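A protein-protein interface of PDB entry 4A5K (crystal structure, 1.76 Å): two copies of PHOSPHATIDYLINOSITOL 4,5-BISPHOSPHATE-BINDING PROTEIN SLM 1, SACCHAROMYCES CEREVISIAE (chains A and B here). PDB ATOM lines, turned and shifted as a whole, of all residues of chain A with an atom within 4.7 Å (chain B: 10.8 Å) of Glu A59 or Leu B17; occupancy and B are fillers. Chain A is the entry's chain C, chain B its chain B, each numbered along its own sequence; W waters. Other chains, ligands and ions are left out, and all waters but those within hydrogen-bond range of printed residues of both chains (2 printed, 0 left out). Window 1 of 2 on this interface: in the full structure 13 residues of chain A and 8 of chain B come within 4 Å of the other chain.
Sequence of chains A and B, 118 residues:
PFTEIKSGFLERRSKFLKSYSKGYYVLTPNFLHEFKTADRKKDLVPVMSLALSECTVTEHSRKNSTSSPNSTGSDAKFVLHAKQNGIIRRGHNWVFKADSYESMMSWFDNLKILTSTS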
ATOM      1  N   ARG A  13       0.445   5.882  14.151  1.00  0.00           N
ATOM      2  CA  ARG A  13      -0.296   6.044  15.387  1.00  0.00           C
ATOM      3  C   ARG A  13      -1.394   5.003  15.502  1.00  0.00           C
ATOM      4  O   ARG A  13      -2.054   4.656  14.512  1.00  0.00           O
ATOM      5  CB  ARG A  13      -0.928   7.439  15.457  1.00  0.00           C
ATOM      6  CG  ARG A  13      -1.344   7.819  16.872  1.00  0.00           C
ATOM      7  CD  ARG A  13      -2.385   8.929  16.879  1.00  0.00           C
ATOM      8  NE  ARG A  13      -1.799  10.244  16.653  1.00  0.00           N
ATOM      9  CZ  ARG A  13      -2.461  11.272  16.133  1.00  0.00           C
ATOM     10  NH1 ARG A  13      -3.728  11.131  15.766  1.00  0.00           N
ATOM     11  NH2 ARG A  13      -1.850  12.439  15.968  1.00  0.00           N
ATOM     12  N   VAL A  57      -4.392  11.129   0.555  1.00  0.00           N
ATOM     13  CA  VAL A  57      -3.682  11.812   1.642  1.00  0.00           C
ATOM     14  C   VAL A  57      -4.283  13.189   1.826  1.00  0.00           C
ATOM     15  O   VAL A  57      -4.402  13.964   0.876  1.00  0.00           O
ATOM     16  CB  VAL A  57      -2.167  11.910   1.412  1.00  0.00           C
ATOM     17  CG1 VAL A  57      -1.510  10.586   1.742  1.00  0.00           C
ATOM     18  CG2 VAL A  57      -1.867  12.345  -0.012  1.00  0.00           C
ATOM     19  N   THR A  58      -4.687  13.482   3.051  1.00  0.00           N
ATOM     20  CA  THR A  58      -5.487  14.667   3.294  1.00  0.00           C
ATOM     21  C   THR A  58      -4.615  15.764   3.891  1.00  0.00           C
ATOM     22  O   THR A  58      -4.137  16.639   3.169  1.00  0.00           O
ATOM     23  CB  THR A  58      -6.753  14.349   4.131  1.00  0.00           C
ATOM     24  OG1 THR A  58      -6.391  13.656   5.329  1.00  0.00           O
ATOM     25  CG2 THR A  58      -7.707  13.467   3.329  1.00  0.00           C
ATOM     26  N   GLU A  59      -4.363  15.714   5.188  1.00  0.00           N
ATOM     27  CA  GLU A  59      -3.570  16.769   5.772  1.00  0.00           C
ATOM     28  C   GLU A  59      -2.161  16.356   6.130  1.00  0.00           C
ATOM     29  O   GLU A  59      -1.828  15.166   6.228  1.00  0.00           O
ATOM     30  CB  GLU A  59      -4.271  17.410   6.973  1.00  0.00           C
ATOM     31  CG  GLU A  59      -4.470  16.523   8.159  1.00  0.00           C
ATOM     32  CD  GLU A  59      -5.382  17.163   9.193  1.00  0.00           C
ATOM     33  OE1 GLU A  59      -5.094  18.295   9.632  1.00  0.00           O
ATOM     34  OE2 GLU A  59      -6.397  16.535   9.554  1.00  0.00           O
ATOM     35  N   HIS A  60      -1.332  17.366   6.322  1.00  0.00           N
ATOM     36  CA  HIS A  60       0.010  17.151   6.827  1.00  0.00           C
ATOM     37  C   HIS A  60       0.424  18.332   7.691  1.00  0.00           C
ATOM     38  O   HIS A  60      -0.180  19.413   7.637  1.00  0.00           O
ATOM     39  CB  HIS A  60       0.986  16.877   5.667  1.00  0.00           C
ATOM     40  CG  HIS A  60       1.203  18.051   4.758  1.00  0.00           C
ATOM     41  ND1 HIS A  60       1.922  19.161   5.144  1.00  0.00           N
ATOM     42  CD2 HIS A  60       0.827  18.273   3.475  1.00  0.00           C
ATOM     43  CE1 HIS A  60       1.969  20.024   4.142  1.00  0.00           C
ATOM     44  NE2 HIS A  60       1.320  19.508   3.115  1.00  0.00           N
ATOM     45  N   SER A  61       1.427  18.107   8.521  1.00  0.00           N
ATOM     46  CA  SER A  61       1.939  19.120   9.416  1.00  0.00           C
ATOM     47  C   SER A  61       2.449  20.303   8.612  1.00  0.00           C
ATOM     48  O   SER A  61       2.935  20.131   7.501  1.00  0.00           O
ATOM     49  CB  SER A  61       3.104  18.538  10.217  1.00  0.00           C
ATOM     50  OG  SER A  61       2.719  17.381  10.954  1.00  0.00           O
ATOM     51  N   LYS A  77       4.118  14.930  10.433  1.00  0.00           N
ATOM     52  CA  LYS A  77       3.007  13.977  10.365  1.00  0.00           C
ATOM     53  C   LYS A  77       2.157  14.155   9.114  1.00  0.00           C
ATOM     54  O   LYS A  77       2.068  15.248   8.555  1.00  0.00           O
ATOM     55  CB  LYS A  77       2.109  14.132  11.605  1.00  0.00           C
ATOM     56  CG  LYS A  77       2.775  13.808  12.910  1.00  0.00           C
ATOM     57  CD  LYS A  77       1.797  14.093  14.054  1.00  0.00           C
ATOM     58  CE  LYS A  77       2.511  14.289  15.374  1.00  0.00           C
ATOM     59  NZ  LYS A  77       1.590  14.826  16.423  1.00  0.00           N
ATOM     60  N   PHE A  78       1.536  13.068   8.665  1.00  0.00           N
ATOM     61  CA  PHE A  78       0.547  13.168   7.616  1.00  0.00           C
ATOM     62  C   PHE A  78      -0.545  12.148   7.853  1.00  0.00           C
ATOM     63  O   PHE A  78      -0.364  11.198   8.627  1.00  0.00           O
ATOM     64  CB  PHE A  78       1.157  12.995   6.209  1.00  0.00           C
ATOM     65  CG  PHE A  78       1.706  11.615   5.923  1.00  0.00           C
ATOM     66  CD1 PHE A  78       3.037  11.309   6.206  1.00  0.00           C
ATOM     67  CD2 PHE A  78       0.909  10.644   5.340  1.00  0.00           C
ATOM     68  CE1 PHE A  78       3.557  10.054   5.928  1.00  0.00           C
ATOM     69  CE2 PHE A  78       1.423   9.387   5.073  1.00  0.00           C
ATOM     70  CZ  PHE A  78       2.750   9.101   5.357  1.00  0.00           C
ATOM     71  N   VAL A  79      -1.661  12.366   7.170  1.00  0.00           N
ATOM     72  CA  VAL A  79      -2.877  11.577   7.337  1.00  0.00           C
ATOM     73  C   VAL A  79      -3.253  10.854   6.054  1.00  0.00           C
ATOM     74  O   VAL A  79      -3.361  11.465   4.990  1.00  0.00           O
ATOM     75  CB  VAL A  79      -4.047  12.497   7.762  1.00  0.00           C
ATOM     76  CG1 VAL A  79      -5.329  11.687   7.940  1.00  0.00           C
ATOM     77  CG2 VAL A  79      -3.679  13.225   9.029  1.00  0.00           C
ATOM     78  N   PHE A 108       4.491  12.462   1.584  1.00  0.00           N
ATOM     79  CA  PHE A 108       3.214  13.068   1.216  1.00  0.00           C
ATOM     80  C   PHE A 108       3.068  13.311  -0.282  1.00  0.00           C
ATOM     81  O   PHE A 108       2.066  12.935  -0.900  1.00  0.00           O
ATOM     82  CB  PHE A 108       3.030  14.404   1.946  1.00  0.00           C
ATOM     83  CG  PHE A 108       1.670  15.015   1.724  1.00  0.00           C
ATOM     84  CD1 PHE A 108       0.590  14.638   2.519  1.00  0.00           C
ATOM     85  CD2 PHE A 108       1.469  15.947   0.711  1.00  0.00           C
ATOM     86  CE1 PHE A 108      -0.668  15.188   2.310  1.00  0.00           C
ATOM     87  CE2 PHE A 108       0.214  16.501   0.498  1.00  0.00           C
ATOM     88  CZ  PHE A 108      -0.852  16.125   1.297  1.00  0.00           C
ATOM     89  N   ARG B  12      -4.501  27.356  15.205  1.00  0.00           N
ATOM     90  CA  ARG B  12      -5.656  26.521  14.865  1.00  0.00           C
ATOM     91  C   ARG B  12      -5.278  25.062  15.045  1.00  0.00           C
ATOM     92  O   ARG B  12      -4.237  24.619  14.565  1.00  0.00           O
ATOM     93  CB  ARG B  12      -6.166  26.772  13.450  1.00  0.00           C
ATOM     94  CG  ARG B  12      -7.403  25.951  13.121  1.00  0.00           C
ATOM     95  CD  ARG B  12      -8.089  26.406  11.845  1.00  0.00           C
ATOM     96  NE  ARG B  12      -7.143  26.756  10.790  1.00  0.00           N
ATOM     97  CZ  ARG B  12      -6.657  25.900   9.899  1.00  0.00           C
ATOM     98  NH1 ARG B  12      -7.020  24.629   9.935  1.00  0.00           N
ATOM     99  NH2 ARG B  12      -5.803  26.314   8.974  1.00  0.00           N
ATOM    100  N   ARG B  13      -6.104  24.319  15.770  1.00  0.00           N
ATOM    101  CA  ARG B  13      -5.765  22.922  16.058  1.00  0.00           C
ATOM    102  C   ARG B  13      -6.146  22.001  14.905  1.00  0.00           C
ATOM    103  O   ARG B  13      -7.173  22.199  14.240  1.00  0.00           O
ATOM    104  CB  ARG B  13      -6.489  22.452  17.332  1.00  0.00           C
ATOM    105  CG  ARG B  13      -5.868  21.188  17.941  1.00  0.00           C
ATOM    106  CD  ARG B  13      -6.564  20.800  19.242  1.00  0.00           C
ATOM    107  NE  ARG B  13      -5.987  19.583  19.811  1.00  0.00           N
ATOM    108  CZ  ARG B  13      -6.529  18.375  19.694  1.00  0.00           C
ATOM    109  NH1 ARG B  13      -7.671  18.219  19.035  1.00  0.00           N
ATOM    110  NH2 ARG B  13      -5.936  17.323  20.241  1.00  0.00           N
ATOM    111  N   SER B  14      -5.317  20.978  14.674  1.00  0.00           N
ATOM    112  CA  SER B  14      -5.665  19.878  13.788  1.00  0.00           C
ATOM    113  C   SER B  14      -6.100  18.706  14.653  1.00  0.00           C
ATOM    114  O   SER B  14      -5.345  18.225  15.500  1.00  0.00           O
ATOM    115  CB  SER B  14      -4.465  19.438  12.937  1.00  0.00           C
ATOM    116  OG  SER B  14      -4.748  18.188  12.309  1.00  0.00           O
ATOM    117  N   LYS B  15      -7.311  18.232  14.424  1.00  0.00           N
ATOM    118  CA  LYS B  15      -7.837  17.109  15.187  1.00  0.00           C
ATOM    119  C   LYS B  15      -6.995  15.851  14.997  1.00  0.00           C
ATOM    120  O   LYS B  15      -6.629  15.200  15.981  1.00  0.00           O
ATOM    121  CB  LYS B  15      -9.309  16.883  14.820  1.00  0.00           C
ATOM    122  CG  LYS B  15      -9.766  15.452  14.619  1.00  0.00           C
ATOM    123  CD  LYS B  15     -11.289  15.433  14.462  1.00  0.00           C
ATOM    124  CE  LYS B  15     -11.781  14.240  13.663  1.00  0.00           C
ATOM    125  NZ  LYS B  15     -13.256  14.300  13.433  1.00  0.00           N
ATOM    126  N   PHE B  16      -6.660  15.530  13.743  1.00  0.00           N
ATOM    127  CA  PHE B  16      -5.920  14.297  13.464  1.00  0.00           C
ATOM    128  C   PHE B  16      -4.437  14.378  13.745  1.00  0.00           C
ATOM    129  O   PHE B  16      -3.854  13.408  14.238  1.00  0.00           O
ATOM    130  CB  PHE B  16      -6.161  13.806  12.037  1.00  0.00           C
ATOM    131  CG  PHE B  16      -7.586  13.434  11.764  1.00  0.00           C
ATOM    132  CD1 PHE B  16      -8.227  12.483  12.539  1.00  0.00           C
ATOM    133  CD2 PHE B  16      -8.284  14.032  10.731  1.00  0.00           C
ATOM    134  CE1 PHE B  16      -9.549  12.140  12.289  1.00  0.00           C
ATOM    135  CE2 PHE B  16      -9.597  13.695  10.476  1.00  0.00           C
ATOM    136  CZ  PHE B  16     -10.229  12.750  11.258  1.00  0.00           C
ATOM    137  N   LEU B  17      -3.816  15.517  13.439  1.00  0.00           N
ATOM    138  CA  LEU B  17      -2.387  15.669  13.690  1.00  0.00           C
ATOM    139  C   LEU B  17      -2.055  15.996  15.146  1.00  0.00           C
ATOM    140  O   LEU B  17      -0.897  15.887  15.560  1.00  0.00           O
ATOM    141  CB  LEU B  17      -1.770  16.725  12.776  1.00  0.00           C
ATOM    142  CG  LEU B  17      -1.946  16.572  11.269  1.00  0.00           C
ATOM    143  CD1 LEU B  17      -1.404  17.812  10.560  1.00  0.00           C
ATOM    144  CD2 LEU B  17      -1.247  15.325  10.777  1.00  0.00           C
ATOM    145  N   LYS B  18      -3.064  16.396  15.915  1.00  0.00           N
ATOM    146  CA  LYS B  18      -2.867  16.772  17.310  1.00  0.00           C
ATOM    147  C   LYS B  18      -1.731  17.769  17.436  1.00  0.00           C
ATOM    148  O   LYS B  18      -0.768  17.558  18.182  1.00  0.00           O
ATOM    149  CB  LYS B  18      -2.596  15.530  18.177  1.00  0.00           C
ATOM    150  CG  LYS B  18      -3.808  14.615  18.329  1.00  0.00           C
ATOM    151  CD  LYS B  18      -3.503  13.416  19.215  1.00  0.00           C
ATOM    152  CE  LYS B  18      -4.786  12.749  19.684  1.00  0.00           C
ATOM    153  NZ  LYS B  18      -5.731  12.523  18.558  1.00  0.00           N
ATOM    154  N   SER B  19      -1.837  18.854  16.673  1.00  0.00           N
ATOM    155  CA  SER B  19      -0.861  19.918  16.725  1.00  0.00           C
ATOM    156  C   SER B  19      -1.571  21.213  16.389  1.00  0.00           C
ATOM    157  O   SER B  19      -2.684  21.198  15.858  1.00  0.00           O
ATOM    158  CB  SER B  19       0.226  19.690  15.682  1.00  0.00           C
ATOM    159  OG  SER B  19      -0.369  19.512  14.418  1.00  0.00           O
ATOM    160  N   TYR B  20      -0.903  22.326  16.672  1.00  0.00           N
ATOM    161  CA  TYR B  20      -1.428  23.638  16.324  1.00  0.00           C
ATOM    162  C   TYR B  20      -0.565  24.257  15.267  1.00  0.00           C
ATOM    163  O   TYR B  20       0.642  24.030  15.217  1.00  0.00           O
ATOM    164  CB  TYR B  20      -1.429  24.585  17.521  1.00  0.00           C
ATOM    165  CG  TYR B  20      -2.531  24.303  18.495  1.00  0.00           C
ATOM    166  CD1 TYR B  20      -2.357  23.366  19.498  1.00  0.00           C
ATOM    167  CD2 TYR B  20      -3.763  24.955  18.392  1.00  0.00           C
ATOM    168  CE1 TYR B  20      -3.363  23.088  20.395  1.00  0.00           C
ATOM    169  CE2 TYR B  20      -4.774  24.686  19.295  1.00  0.00           C
ATOM    170  CZ  TYR B  20      -4.564  23.742  20.287  1.00  0.00           C
ATOM    171  OH  TYR B  20      -5.559  23.450  21.190  1.00  0.00           O
ATOM    172  N   SER B  21      -1.199  25.048  14.421  1.00  0.00           N
ATOM    173  CA  SER B  21      -0.464  25.861  13.473  1.00  0.00           C
ATOM    174  C   SER B  21      -0.910  27.320  13.550  1.00  0.00           C
ATOM    175  O   SER B  21      -2.097  27.618  13.492  1.00  0.00           O
ATOM    176  CB  SER B  21      -0.643  25.335  12.061  1.00  0.00           C
ATOM    177  OG  SER B  21       0.113  26.139  11.168  1.00  0.00           O
ATOM    178  N   MET B  48      -7.537  30.754   3.384  1.00  0.00           N
ATOM    179  CA  MET B  48      -8.904  30.251   3.398  1.00  0.00           C
ATOM    180  C   MET B  48      -9.855  31.300   3.953  1.00  0.00           C
ATOM    181  O   MET B  48      -9.448  32.205   4.676  1.00  0.00           O
ATOM    182  CB  MET B  48      -9.012  28.972   4.214  1.00  0.00           C
ATOM    183  CG  MET B  48      -8.594  29.122   5.660  1.00  0.00           C
ATOM    184  SD  MET B  48      -9.179  27.772   6.713  1.00  0.00           S
ATOM    185  CE  MET B  48      -8.595  28.320   8.317  1.00  0.00           C
ATOM    186  N   ILE B  87     -15.477  25.001   4.052  1.00  0.00           N
ATOM    187  CA  ILE B  87     -14.109  24.726   4.476  1.00  0.00           C
ATOM    188  C   ILE B  87     -14.137  23.616   5.521  1.00  0.00           C
ATOM    189  O   ILE B  87     -13.275  22.725   5.541  1.00  0.00           O
ATOM    190  CB  ILE B  87     -13.460  25.982   5.081  1.00  0.00           C
ATOM    191  CG1 ILE B  87     -13.480  27.142   4.077  1.00  0.00           C
ATOM    192  CG2 ILE B  87     -12.041  25.673   5.569  1.00  0.00           C
ATOM    193  CD1 ILE B  87     -12.634  26.930   2.849  1.00  0.00           C
ATOM    194  N   HIS B  92     -19.004  19.752  11.925  1.00  0.00           N
ATOM    195  CA  HIS B  92     -17.653  19.619  12.488  1.00  0.00           C
ATOM    196  C   HIS B  92     -17.193  20.902  13.163  1.00  0.00           C
ATOM    197  O   HIS B  92     -17.845  21.937  13.067  1.00  0.00           O
ATOM    198  CB  HIS B  92     -16.648  19.187  11.423  1.00  0.00           C
ATOM    199  CG  HIS B  92     -16.706  17.724  11.102  1.00  0.00           C
ATOM    200  ND1 HIS B  92     -17.875  17.089  10.741  1.00  0.00           N
ATOM    201  CD2 HIS B  92     -15.740  16.776  11.085  1.00  0.00           C
ATOM    202  CE1 HIS B  92     -17.628  15.810  10.517  1.00  0.00           C
ATOM    203  NE2 HIS B  92     -16.340  15.593  10.721  1.00  0.00           N
ATOM    204  N   ASN B  93     -16.053  20.817  13.839  1.00  0.00           N
ATOM    205  CA  ASN B  93     -15.635  21.831  14.784  1.00  0.00           C
ATOM    206  C   ASN B  93     -14.154  22.115  14.646  1.00  0.00           C
ATOM    207  O   ASN B  93     -13.350  21.203  14.482  1.00  0.00           O
ATOM    208  CB  ASN B  93     -15.939  21.365  16.212  1.00  0.00           C
ATOM    209  CG  ASN B  93     -17.429  21.157  16.454  1.00  0.00           C
ATOM    210  OD1 ASN B  93     -18.181  22.117  16.610  1.00  0.00           O
ATOM    211  ND2 ASN B  93     -17.859  19.899  16.482  1.00  0.00           N
ATOM    212  N   TRP B  94     -13.796  23.390  14.715  1.00  0.00           N
ATOM    213  CA  TRP B  94     -12.406  23.789  14.683  1.00  0.00           C
ATOM    214  C   TRP B  94     -12.095  24.481  16.000  1.00  0.00           C
ATOM    215  O   TRP B  94     -12.894  25.276  16.488  1.00  0.00           O
ATOM    216  CB  TRP B  94     -12.160  24.725  13.499  1.00  0.00           C
ATOM    217  CG  TRP B  94     -11.843  23.979  12.220  1.00  0.00           C
ATOM    218  CD1 TRP B  94     -11.944  22.634  12.005  1.00  0.00           C
ATOM    219  CD2 TRP B  94     -11.381  24.546  10.988  1.00  0.00           C
ATOM    220  NE1 TRP B  94     -11.571  22.328  10.715  1.00  0.00           N
ATOM    221  CE2 TRP B  94     -11.218  23.486  10.073  1.00  0.00           C
ATOM    222  CE3 TRP B  94     -11.088  25.847  10.571  1.00  0.00           C
ATOM    223  CZ2 TRP B  94     -10.775  23.688   8.767  1.00  0.00           C
ATOM    224  CZ3 TRP B  94     -10.647  26.046   9.275  1.00  0.00           C
ATOM    225  CH2 TRP B  94     -10.493  24.971   8.391  1.00  0.00           C
ATOM    226  N   VAL B  95     -10.956  24.155  16.592  1.00  0.00           N
ATOM    227  CA  VAL B  95     -10.544  24.786  17.842  1.00  0.00           C
ATOM    228  C   VAL B  95      -9.436  25.786  17.604  1.00  0.00           C
ATOM    229  O   VAL B  95      -8.439  25.464  16.953  1.00  0.00           O
ATOM    230  CB  VAL B  95     -10.058  23.720  18.846  1.00  0.00           C
ATOM    231  CG1 VAL B  95      -9.502  24.376  20.102  1.00  0.00           C
ATOM    232  CG2 VAL B  95     -11.218  22.777  19.174  1.00  0.00           C
HETATM  233  O   HOH W   1       1.578  17.737  13.534  1.00  0.00           O
HETATM  234  O   HOH W   2      -7.837  16.927  11.554  1.00  0.00           O
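Among the printed residues, pairs that only touch across the chains: Arg A13 with Leu B17, Arg A13 with Lys B18, Glu A59 with Phe B16, Glu A59 with Leu B17, His A60 with Leu B17, Ser A61 with Leu B17, Val A79 with Phe B16 and Val A79 with Leu B17.
Water W2 lies within hydrogen-bond range of the side-chain carboxylate (OE2) of Glu A59 (2.5 Å), the backbone NH (N) of Phe B16 (2.9 Å), the backbone NH (N) of Lys B15 (3.2 Å) and the side-chain hydroxyl (OG) of Ser B14 (3.4 Å). Water W1 lies within hydrogen-bond range of OG of Ser B19 (2.8 Å) and OG of Ser A61 (2.8 Å).
1 position is printed for both chains. Of the 11 pairs that touch across the chains among the printed residues, none has its exchanged pair printed and touching as well.
Of chain A, only Arg A13 (3.6 Å), Glu A59 (3.8 Å), His A60 (3.4 Å), Ser A61 (3.5 Å), Lys A77 (2.8 Å) and Val A79 (3.7 Å) come within 4 Å of Leu B17. No residue of chain B comes within 4 Å of Val A57. Of chain B, only Leu B17 (3.4 Å) comes within 4 Å of His A60. Ser A61 touches one residue of chain B. Val A79 touches just these residues of chain B: Phe B16 (3.9 Å) and Leu B17 (3.7 Å). Printed residues of chain A within 4 Å of Phe B16: Arg A13, Glu A59 and Val A79. Printed residues of chain A within 4 Å of Ser B14: Glu A59. The nearest printed residue of chain A that does not touch Lys B18 is Lys A77 (4.01 Å).
The backbone NH of Leu B17 sits at hydrogen-bond distance from the side-chain hydroxyl of Ser B14 (3.0 Å). N of Ser B14 is in hydrogen-bond range of O of Ser B19, 2.9 Å away. N of Thr A58 sits at hydrogen-bond distance from O of Val A79 (3.1 Å). O of Glu A59 is in hydrogen-bond range of N of Val A79, 3.0 Å away. The side-chain hydroxyl of Ser A61 sits at hydrogen-bond distance from the backbone NH of Lys A77.
Hydrophobic or aromatic side chains of chain B within 4 Å of the printed part of chain A: Phe B16 and Leu B17. Of the 10 printed residues of chain A, 6 touch a printed residue of chain B. Printed residues of chain A that touch a printed residue of chain B: Arg A13, Glu A59, His A60, Ser A61, Lys A77 and Val A79.
The side-chain hydroxyl of Ser B14 is in hydrogen-bond range of the side-chain carboxylate of Glu A59, 2.7 Å away. O of Phe B16 is in hydrogen-bond range of NH1 of Arg A13, 2.7 Å away. The side-chain amino group (NZ) of Lys A77 sits at hydrogen-bond distance from the backbone carbonyl oxygen (O) of Leu B17 (2.8 Å).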
